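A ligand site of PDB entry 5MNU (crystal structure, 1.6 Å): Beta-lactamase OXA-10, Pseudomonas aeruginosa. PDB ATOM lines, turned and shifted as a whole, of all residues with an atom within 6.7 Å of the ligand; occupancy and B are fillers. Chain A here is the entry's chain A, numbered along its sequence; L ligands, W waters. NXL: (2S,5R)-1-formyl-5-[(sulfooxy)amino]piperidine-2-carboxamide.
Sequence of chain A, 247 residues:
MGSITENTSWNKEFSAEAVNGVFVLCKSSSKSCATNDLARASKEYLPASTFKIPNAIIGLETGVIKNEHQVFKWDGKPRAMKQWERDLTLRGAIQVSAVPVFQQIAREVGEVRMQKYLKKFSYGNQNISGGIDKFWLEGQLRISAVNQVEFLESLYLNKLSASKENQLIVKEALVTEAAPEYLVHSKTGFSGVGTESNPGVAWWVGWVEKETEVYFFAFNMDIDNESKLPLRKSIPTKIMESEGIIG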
ATOM      1  N   PRO A  47      13.282  21.421 -16.448  1.00  0.00           N
ATOM      2  CA  PRO A  47      13.804  20.696 -15.270  1.00  0.00           C
ATOM      3  C   PRO A  47      12.959  20.906 -14.023  1.00  0.00           C
ATOM      4  O   PRO A  47      12.926  20.016 -13.171  1.00  0.00           O
ATOM      5  CB  PRO A  47      15.214  21.263 -15.082  1.00  0.00           C
ATOM      6  CG  PRO A  47      15.534  21.982 -16.332  1.00  0.00           C
ATOM      7  CD  PRO A  47      14.253  22.413 -16.953  1.00  0.00           C
ATOM      8  N   ALA A  48      12.305  22.048 -13.883  1.00  0.00           N
ATOM      9  CA  ALA A  48      11.611  22.395 -12.642  1.00  0.00           C
ATOM     10  C   ALA A  48      12.546  22.194 -11.441  1.00  0.00           C
ATOM     11  O   ALA A  48      13.719  22.549 -11.519  1.00  0.00           O
ATOM     12  CB  ALA A  48      10.335  21.594 -12.509  1.00  0.00           C
ATOM     13  N   SER A  49      12.036  21.621 -10.346  1.00  0.00           N
ATOM     14  CA  SER A  49      12.803  21.570  -9.120  1.00  0.00           C
ATOM     15  C   SER A  49      14.067  20.684  -9.188  1.00  0.00           C
ATOM     16  O   SER A  49      14.893  20.757  -8.306  1.00  0.00           O
ATOM     17  CB  SER A  49      11.975  21.062  -7.906  1.00  0.00           C
ATOM     18  OG  SER A  49      11.109  22.142  -7.529  1.00  0.00           O
ATOM     19  N   THR A  50      14.193  19.846 -10.207  1.00  0.00           N
ATOM     20  CA  THR A  50      15.412  19.044 -10.312  1.00  0.00           C
ATOM     21  C   THR A  50      16.580  19.960 -10.625  1.00  0.00           C
ATOM     22  O   THR A  50      17.739  19.563 -10.466  1.00  0.00           O
ATOM     23  CB  THR A  50      15.313  17.928 -11.388  1.00  0.00           C
ATOM     24  OG1 THR A  50      15.257  18.490 -12.704  1.00  0.00           O
ATOM     25  CG2 THR A  50      14.103  17.032 -11.141  1.00  0.00           C
ATOM     26  N   LYS A  52      17.465  22.320  -8.855  1.00  0.00           N
ATOM     27  CA  LYS A  52      18.155  22.656  -7.617  1.00  0.00           C
ATOM     28  C   LYS A  52      19.497  21.945  -7.496  1.00  0.00           C
ATOM     29  O   LYS A  52      20.380  22.441  -6.793  1.00  0.00           O
ATOM     30  CB  LYS A  52      17.281  22.329  -6.413  1.00  0.00           C
ATOM     31  CG  LYS A  52      16.072  23.259  -6.263  1.00  0.00           C
ATOM     32  CD  LYS A  52      15.423  23.140  -4.888  1.00  0.00           C
ATOM     33  CE  LYS A  52      14.366  24.227  -4.686  1.00  0.00           C
ATOM     34  NZ  LYS A  52      13.103  23.823  -5.336  1.00  0.00           N
ATOM     35  N   MET A  81       4.425  28.517  -0.564  1.00  0.00           N
ATOM     36  CA  MET A  81       4.146  27.312   0.207  1.00  0.00           C
ATOM     37  C   MET A  81       4.548  27.557   1.653  1.00  0.00           C
ATOM     38  O   MET A  81       5.631  28.074   1.919  1.00  0.00           O
ATOM     39  CB  MET A  81       4.900  26.099  -0.338  1.00  0.00           C
ATOM     40  CG  MET A  81       4.673  25.880  -1.815  1.00  0.00           C
ATOM     41  SD  MET A  81       5.033  24.205  -2.345  1.00  0.00           S
ATOM     42  CE  MET A  81       4.146  24.174  -3.899  1.00  0.00           C
ATOM     43  N   GLN A  83       5.578  25.602   3.920  1.00  0.00           N
ATOM     44  CA  GLN A  83       6.784  24.935   4.364  1.00  0.00           C
ATOM     45  C   GLN A  83       8.048  25.708   4.037  1.00  0.00           C
ATOM     46  O   GLN A  83       9.110  25.369   4.561  1.00  0.00           O
ATOM     47  CB  GLN A  83       6.882  23.541   3.747  1.00  0.00           C
ATOM     48  CG  GLN A  83       6.750  23.513   2.242  1.00  0.00           C
ATOM     49  CD  GLN A  83       5.334  23.205   1.800  1.00  0.00           C
ATOM     50  OE1 GLN A  83       4.356  23.743   2.338  1.00  0.00           O
ATOM     51  NE2 GLN A  83       5.209  22.315   0.824  1.00  0.00           N
ATOM     52  N   TRP A  84       7.970  26.729   3.174  1.00  0.00           N
ATOM     53  CA  TRP A  84       9.106  27.578   2.850  1.00  0.00           C
ATOM     54  C   TRP A  84       9.234  28.777   3.767  1.00  0.00           C
ATOM     55  O   TRP A  84      10.219  29.524   3.642  1.00  0.00           O
ATOM     56  CB  TRP A  84       9.006  28.094   1.407  1.00  0.00           C
ATOM     57  CG  TRP A  84       8.854  27.055   0.342  1.00  0.00           C
ATOM     58  CD1 TRP A  84       9.087  25.730   0.437  1.00  0.00           C
ATOM     59  CD2 TRP A  84       8.412  27.284  -1.002  1.00  0.00           C
ATOM     60  NE1 TRP A  84       8.828  25.097  -0.759  1.00  0.00           N
ATOM     61  CE2 TRP A  84       8.408  26.045  -1.663  1.00  0.00           C
ATOM     62  CE3 TRP A  84       8.025  28.427  -1.717  1.00  0.00           C
ATOM     63  CZ2 TRP A  84       8.036  25.900  -3.002  1.00  0.00           C
ATOM     64  CZ3 TRP A  84       7.644  28.284  -3.044  1.00  0.00           C
ATOM     65  CH2 TRP A  84       7.660  27.039  -3.673  1.00  0.00           C
ATOM     66  N   ILE A  94      16.699  22.374  -0.236  1.00  0.00           N
ATOM     67  CA  ILE A  94      16.543  21.396  -1.313  1.00  0.00           C
ATOM     68  C   ILE A  94      15.411  20.419  -0.982  1.00  0.00           C
ATOM     69  O   ILE A  94      14.554  20.125  -1.814  1.00  0.00           O
ATOM     70  CB  ILE A  94      17.880  20.662  -1.564  1.00  0.00           C
ATOM     71  CG1 ILE A  94      18.899  21.610  -2.201  1.00  0.00           C
ATOM     72  CG2 ILE A  94      17.662  19.427  -2.451  1.00  0.00           C
ATOM     73  CD1 ILE A  94      20.329  21.064  -2.238  1.00  0.00           C
ATOM     74  N   GLN A  95      15.382  19.927   0.256  1.00  0.00           N
ATOM     75  CA  GLN A  95      14.444  18.878   0.636  1.00  0.00           C
ATOM     76  C   GLN A  95      13.002  19.402   0.651  1.00  0.00           C
ATOM     77  O   GLN A  95      12.104  18.717   0.168  1.00  0.00           O
ATOM     78  CB  GLN A  95      14.824  18.306   1.986  1.00  0.00           C
ATOM     79  CG  GLN A  95      16.147  17.539   1.991  1.00  0.00           C
ATOM     80  CD  GLN A  95      16.024  16.131   1.440  1.00  0.00           C
ATOM     81  OE1 GLN A  95      14.994  15.479   1.622  1.00  0.00           O
ATOM     82  NE2 GLN A  95      17.060  15.660   0.767  1.00  0.00           N
ATOM     83  N   VAL A  96      12.770  20.587   1.212  1.00  0.00           N
ATOM     84  CA  VAL A  96      11.420  21.168   1.134  1.00  0.00           C
ATOM     85  C   VAL A  96      11.210  21.884  -0.185  1.00  0.00           C
ATOM     86  O   VAL A  96      10.074  22.332  -0.466  1.00  0.00           O
ATOM     87  CB  VAL A  96      11.105  22.147   2.294  1.00  0.00           C
ATOM     88  CG1 VAL A  96      11.401  21.492   3.627  1.00  0.00           C
ATOM     89  CG2 VAL A  96      11.851  23.477   2.143  1.00  0.00           C
ATOM     90  N   SER A  97      12.261  22.015  -0.992  1.00  0.00           N
ATOM     91  CA  SER A  97      12.193  22.496  -2.373  1.00  0.00           C
ATOM     92  C   SER A  97      11.734  23.957  -2.438  1.00  0.00           C
ATOM     93  O   SER A  97      10.800  24.307  -3.153  1.00  0.00           O
ATOM     94  CB  SER A  97      11.301  21.578  -3.211  1.00  0.00           C
ATOM     95  OG  SER A  97      11.797  21.521  -4.532  1.00  0.00           O
ATOM     96  N   ALA A  98      12.439  24.807  -1.681  1.00  0.00           N
ATOM     97  CA  ALA A  98      12.091  26.218  -1.506  1.00  0.00           C
ATOM     98  C   ALA A  98      12.552  27.022  -2.717  1.00  0.00           C
ATOM     99  O   ALA A  98      13.659  27.558  -2.758  1.00  0.00           O
ATOM    100  CB  ALA A  98      12.682  26.766  -0.215  1.00  0.00           C
ATOM    101  N   VAL A  99      11.649  27.139  -3.683  1.00  0.00           N
ATOM    102  CA  VAL A  99      11.926  27.898  -4.909  1.00  0.00           C
ATOM    103  C   VAL A  99      12.547  29.272  -4.652  1.00  0.00           C
ATOM    104  O   VAL A  99      13.572  29.584  -5.266  1.00  0.00           O
ATOM    105  CB  VAL A  99      10.658  27.988  -5.767  1.00  0.00           C
ATOM    106  CG1 VAL A  99      10.871  28.890  -6.973  1.00  0.00           C
ATOM    107  CG2 VAL A  99      10.207  26.589  -6.197  1.00  0.00           C
ATOM    108  N   LEU A 137      11.998  27.141 -14.717  1.00  0.00           N
ATOM    109  CA  LEU A 137      10.629  27.023 -14.250  1.00  0.00           C
ATOM    110  C   LEU A 137       9.620  27.233 -15.366  1.00  0.00           C
ATOM    111  O   LEU A 137       8.620  26.506 -15.453  1.00  0.00           O
ATOM    112  CB  LEU A 137      10.363  28.048 -13.150  1.00  0.00           C
ATOM    113  CG  LEU A 137      11.220  27.944 -11.897  1.00  0.00           C
ATOM    114  CD1 LEU A 137      10.997  29.151 -10.996  1.00  0.00           C
ATOM    115  CD2 LEU A 137      10.915  26.650 -11.172  1.00  0.00           C
ATOM    116  N   LYS A 187      15.722  13.628  -6.075  1.00  0.00           N
ATOM    117  CA  LYS A 187      15.049  14.921  -6.111  1.00  0.00           C
ATOM    118  C   LYS A 187      13.818  14.811  -7.004  1.00  0.00           C
ATOM    119  O   LYS A 187      13.900  14.268  -8.112  1.00  0.00           O
ATOM    120  CB  LYS A 187      15.980  16.012  -6.615  1.00  0.00           C
ATOM    121  CG  LYS A 187      15.391  17.434  -6.598  1.00  0.00           C
ATOM    122  CD  LYS A 187      15.164  17.913  -5.155  1.00  0.00           C
ATOM    123  CE  LYS A 187      14.358  19.202  -5.100  1.00  0.00           C
ATOM    124  NZ  LYS A 187      12.879  18.946  -5.127  1.00  0.00           N
ATOM    125  N   THR A 188      12.695  15.337  -6.512  1.00  0.00           N
ATOM    126  CA  THR A 188      11.444  15.425  -7.262  1.00  0.00           C
ATOM    127  C   THR A 188      11.352  16.776  -7.982  1.00  0.00           C
ATOM    128  O   THR A 188      12.062  17.733  -7.673  1.00  0.00           O
ATOM    129  CB  THR A 188      10.250  15.279  -6.325  1.00  0.00           C
ATOM    130  OG1 THR A 188      10.428  16.149  -5.198  1.00  0.00           O
ATOM    131  CG2 THR A 188      10.080  13.843  -5.830  1.00  0.00           C
ATOM    132  N   GLY A 189      10.427  16.857  -8.941  1.00  0.00           N
ATOM    133  CA  GLY A 189      10.090  18.117  -9.580  1.00  0.00           C
ATOM    134  C   GLY A 189       8.689  18.076 -10.144  1.00  0.00           C
ATOM    135  O   GLY A 189       8.130  17.007 -10.392  1.00  0.00           O
ATOM    136  N   PHE A 190       8.125  19.271 -10.357  1.00  0.00           N
ATOM    137  CA  PHE A 190       6.755  19.412 -10.834  1.00  0.00           C
ATOM    138  C   PHE A 190       6.628  20.797 -11.463  1.00  0.00           C
ATOM    139  O   PHE A 190       6.573  21.798 -10.751  1.00  0.00           O
ATOM    140  CB  PHE A 190       5.768  19.234  -9.681  1.00  0.00           C
ATOM    141  CG  PHE A 190       4.318  19.474 -10.031  1.00  0.00           C
ATOM    142  CD1 PHE A 190       3.773  19.040 -11.223  1.00  0.00           C
ATOM    143  CD2 PHE A 190       3.484  20.099  -9.106  1.00  0.00           C
ATOM    144  CE1 PHE A 190       2.418  19.254 -11.503  1.00  0.00           C
ATOM    145  CE2 PHE A 190       2.152  20.311  -9.378  1.00  0.00           C
ATOM    146  CZ  PHE A 190       1.614  19.887 -10.576  1.00  0.00           C
ATOM    147  N   SER A 191       6.574  20.860 -12.800  1.00  0.00           N
ATOM    148  CA  SER A 191       6.539  22.162 -13.456  1.00  0.00           C
ATOM    149  C   SER A 191       5.174  22.847 -13.354  1.00  0.00           C
ATOM    150  O   SER A 191       5.100  24.072 -13.514  1.00  0.00           O
ATOM    151  CB  SER A 191       6.933  22.046 -14.931  1.00  0.00           C
ATOM    152  OG  SER A 191       5.902  21.447 -15.719  1.00  0.00           O
ATOM    153  N   GLY A 192       4.123  22.090 -13.082  1.00  0.00           N
ATOM    154  CA  GLY A 192       2.760  22.584 -13.026  1.00  0.00           C
ATOM    155  C   GLY A 192       1.864  21.726 -13.877  1.00  0.00           C
ATOM    156  O   GLY A 192       2.270  20.681 -14.393  1.00  0.00           O
ATOM    157  N   TRP A 203       8.836  15.037 -12.339  1.00  0.00           N
ATOM    158  CA  TRP A 203      10.115  14.332 -12.341  1.00  0.00           C
ATOM    159  C   TRP A 203      10.349  13.601 -11.021  1.00  0.00           C
ATOM    160  O   TRP A 203       9.935  14.058  -9.962  1.00  0.00           O
ATOM    161  CB  TRP A 203      11.297  15.288 -12.487  1.00  0.00           C
ATOM    162  CG  TRP A 203      11.551  15.962 -13.783  1.00  0.00           C
ATOM    163  CD1 TRP A 203      11.128  17.207 -14.150  1.00  0.00           C
ATOM    164  CD2 TRP A 203      12.364  15.476 -14.858  1.00  0.00           C
ATOM    165  NE1 TRP A 203      11.615  17.522 -15.401  1.00  0.00           N
ATOM    166  CE2 TRP A 203      12.372  16.472 -15.858  1.00  0.00           C
ATOM    167  CE3 TRP A 203      13.069  14.287 -15.077  1.00  0.00           C
ATOM    168  CZ2 TRP A 203      13.063  16.315 -17.054  1.00  0.00           C
ATOM    169  CZ3 TRP A 203      13.752  14.132 -16.262  1.00  0.00           C
ATOM    170  CH2 TRP A 203      13.742  15.141 -17.242  1.00  0.00           C
ATOM    171  N   LEU A 229       0.230  13.433  -9.081  1.00  0.00           N
ATOM    172  CA  LEU A 229       1.648  13.671  -8.807  1.00  0.00           C
ATOM    173  C   LEU A 229       2.350  12.496  -8.114  1.00  0.00           C
ATOM    174  O   LEU A 229       3.505  12.213  -8.469  1.00  0.00           O
ATOM    175  CB  LEU A 229       1.781  14.950  -7.978  1.00  0.00           C
ATOM    176  CG  LEU A 229       3.165  15.601  -7.874  1.00  0.00           C
ATOM    177  CD1 LEU A 229       3.746  15.948  -9.229  1.00  0.00           C
ATOM    178  CD2 LEU A 229       3.060  16.862  -7.005  1.00  0.00           C
ATOM    179  N   ARG A 232       4.808   9.883  -9.845  1.00  0.00           N
ATOM    180  CA  ARG A 232       6.202  10.120 -10.210  1.00  0.00           C
ATOM    181  C   ARG A 232       7.163   9.334  -9.325  1.00  0.00           C
ATOM    182  O   ARG A 232       8.317   9.123  -9.720  1.00  0.00           O
ATOM    183  CB  ARG A 232       6.534  11.610 -10.144  1.00  0.00           C
ATOM    184  CG  ARG A 232       6.628  12.135  -8.723  1.00  0.00           C
ATOM    185  CD  ARG A 232       6.633  13.636  -8.658  1.00  0.00           C
ATOM    186  NE  ARG A 232       6.467  14.083  -7.289  1.00  0.00           N
ATOM    187  CZ  ARG A 232       6.675  15.318  -6.859  1.00  0.00           C
ATOM    188  NH1 ARG A 232       6.473  15.603  -5.583  1.00  0.00           N
ATOM    189  NH2 ARG A 232       7.066  16.266  -7.701  1.00  0.00           N
HETATM  190  OAC NXL L   1       9.587  21.405  -9.080  1.00  0.00           O
HETATM  191  CAN NXL L   1       9.865  22.108  -8.133  1.00  0.00           C
HETATM  192  N   NXL L   1       8.892  22.985  -7.535  1.00  0.00           N
HETATM  193  CAJ NXL L   1       9.009  23.428  -6.084  1.00  0.00           C
HETATM  194  CA  NXL L   1       7.477  22.918  -8.009  1.00  0.00           C
HETATM  195  C   NXL L   1       7.123  24.391  -8.185  1.00  0.00           C
HETATM  196  O   NXL L   1       7.925  25.115  -8.639  1.00  0.00           O
HETATM  197  NAA NXL L   1       5.812  24.884  -7.798  1.00  0.00           N
HETATM  198  CB  NXL L   1       6.563  22.136  -7.042  1.00  0.00           C
HETATM  199  CAH NXL L   1       6.804  22.416  -5.592  1.00  0.00           C
HETATM  200  CAO NXL L   1       8.244  22.460  -5.201  1.00  0.00           C
HETATM  201  NAK NXL L   1       8.852  21.138  -5.447  1.00  0.00           N
HETATM  202  OAL NXL L   1       8.233  20.225  -4.612  1.00  0.00           O
HETATM  203  SAR NXL L   1       8.357  18.763  -5.381  1.00  0.00           S
HETATM  204  OAD NXL L   1       9.780  18.469  -5.725  1.00  0.00           O
HETATM  205  OAE NXL L   1       7.708  17.731  -4.460  1.00  0.00           O
HETATM  206  OAG NXL L   1       7.713  18.809  -6.747  1.00  0.00           O
HETATM  207  O   HOH W   1       4.141  23.326 -10.076  1.00  0.00           O
HETATM  208  O   HOH W   2      10.664  24.337  -9.592  1.00  0.00           O
HETATM  209  O   HOH W   3       6.984  26.578 -10.911  1.00  0.00           O
HETATM  210  O   HOH W   4       9.229  18.090  -2.146  1.00  0.00           O
HETATM  211  O   HOH W   5       4.126  26.802  -8.329  1.00  0.00           O
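N of Ser 49 sits close to OAC of the ligand, 2.8 Å away.
The side-chain hydroxyl (OG) of Ser 49 is covalently linked to a carbon (CAN) of the ligand, at 1.4 Å.
O of Thr 188 sits close to OAD of the ligand (3.1 Å).
An oxygen (OAD) of the ligand lies within hydrogen-bond range of the side-chain hydroxyl of Thr 188.
The guanidinium group of Arg 232 lies within salt-bridge range of an oxygen (OAE) of the ligand.
The backbone NH (N) of Phe 190 lies within hydrogen-bond range of an oxygen (OAC) of the ligand (2.9 Å).
NAK of the ligand is in hydrogen-bond range of OG of Ser 97 (3.1 Å).
NZ of Lys 187 lies within salt-bridge range of OAD of the ligand, at 3.2 Å.
OG of Ser 49 is in hydrogen-bond range of OG of Ser 97 (3.1 Å).
NZ of Lys 52 lies within hydrogen-bond range of OG of Ser 49.
The guanidinium group (NH2) of Arg 232 is in hydrogen-bond range of the backbone carbonyl oxygen (O) of Gly 189 (3.0 Å).
The side-chain hydroxyl of Ser 97 sits at hydrogen-bond distance from the side-chain amino group of Lys 187, at 2.9 Å.
NE1 of Trp 84 lies close to O of Ser 97 (3.2 Å).
OG of Ser 97 lies within hydrogen-bond range of NZ of Lys 52 (2.8 Å).
N of Trp 203 is in hydrogen-bond range of O of Gly 189, 2.9 Å away.
The side-chain amide nitrogen of Gln 83 sits at hydrogen-bond distance from the side-chain sulfur of Met 81.
Residues that only touch the ligand: Ala 48, Met 81, Val 99 and Gly 189.
Hydrophobic or aromatic side chains that line the ligand: Ala 48, Met 81, Val 99 and Phe 190.
Within 4 Å of the ligand: Ala 48, Ser 49, Met 81, Ser 97, Val 99, Lys 187, Thr 188, Gly 189, Phe 190 and Arg 232.
The nearest printed residue that does not touch the ligand is Trp 84 (4.1 Å).
Water W2 lies within hydrogen-bond range of an oxygen (O) of the ligand (3.0 Å) and the side-chain hydroxyl (OG) of Ser 49 (3.0 Å).
Water W1 lies within hydrogen-bond range of O of Phe 190, NAA of the ligand and N of Gly 192.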
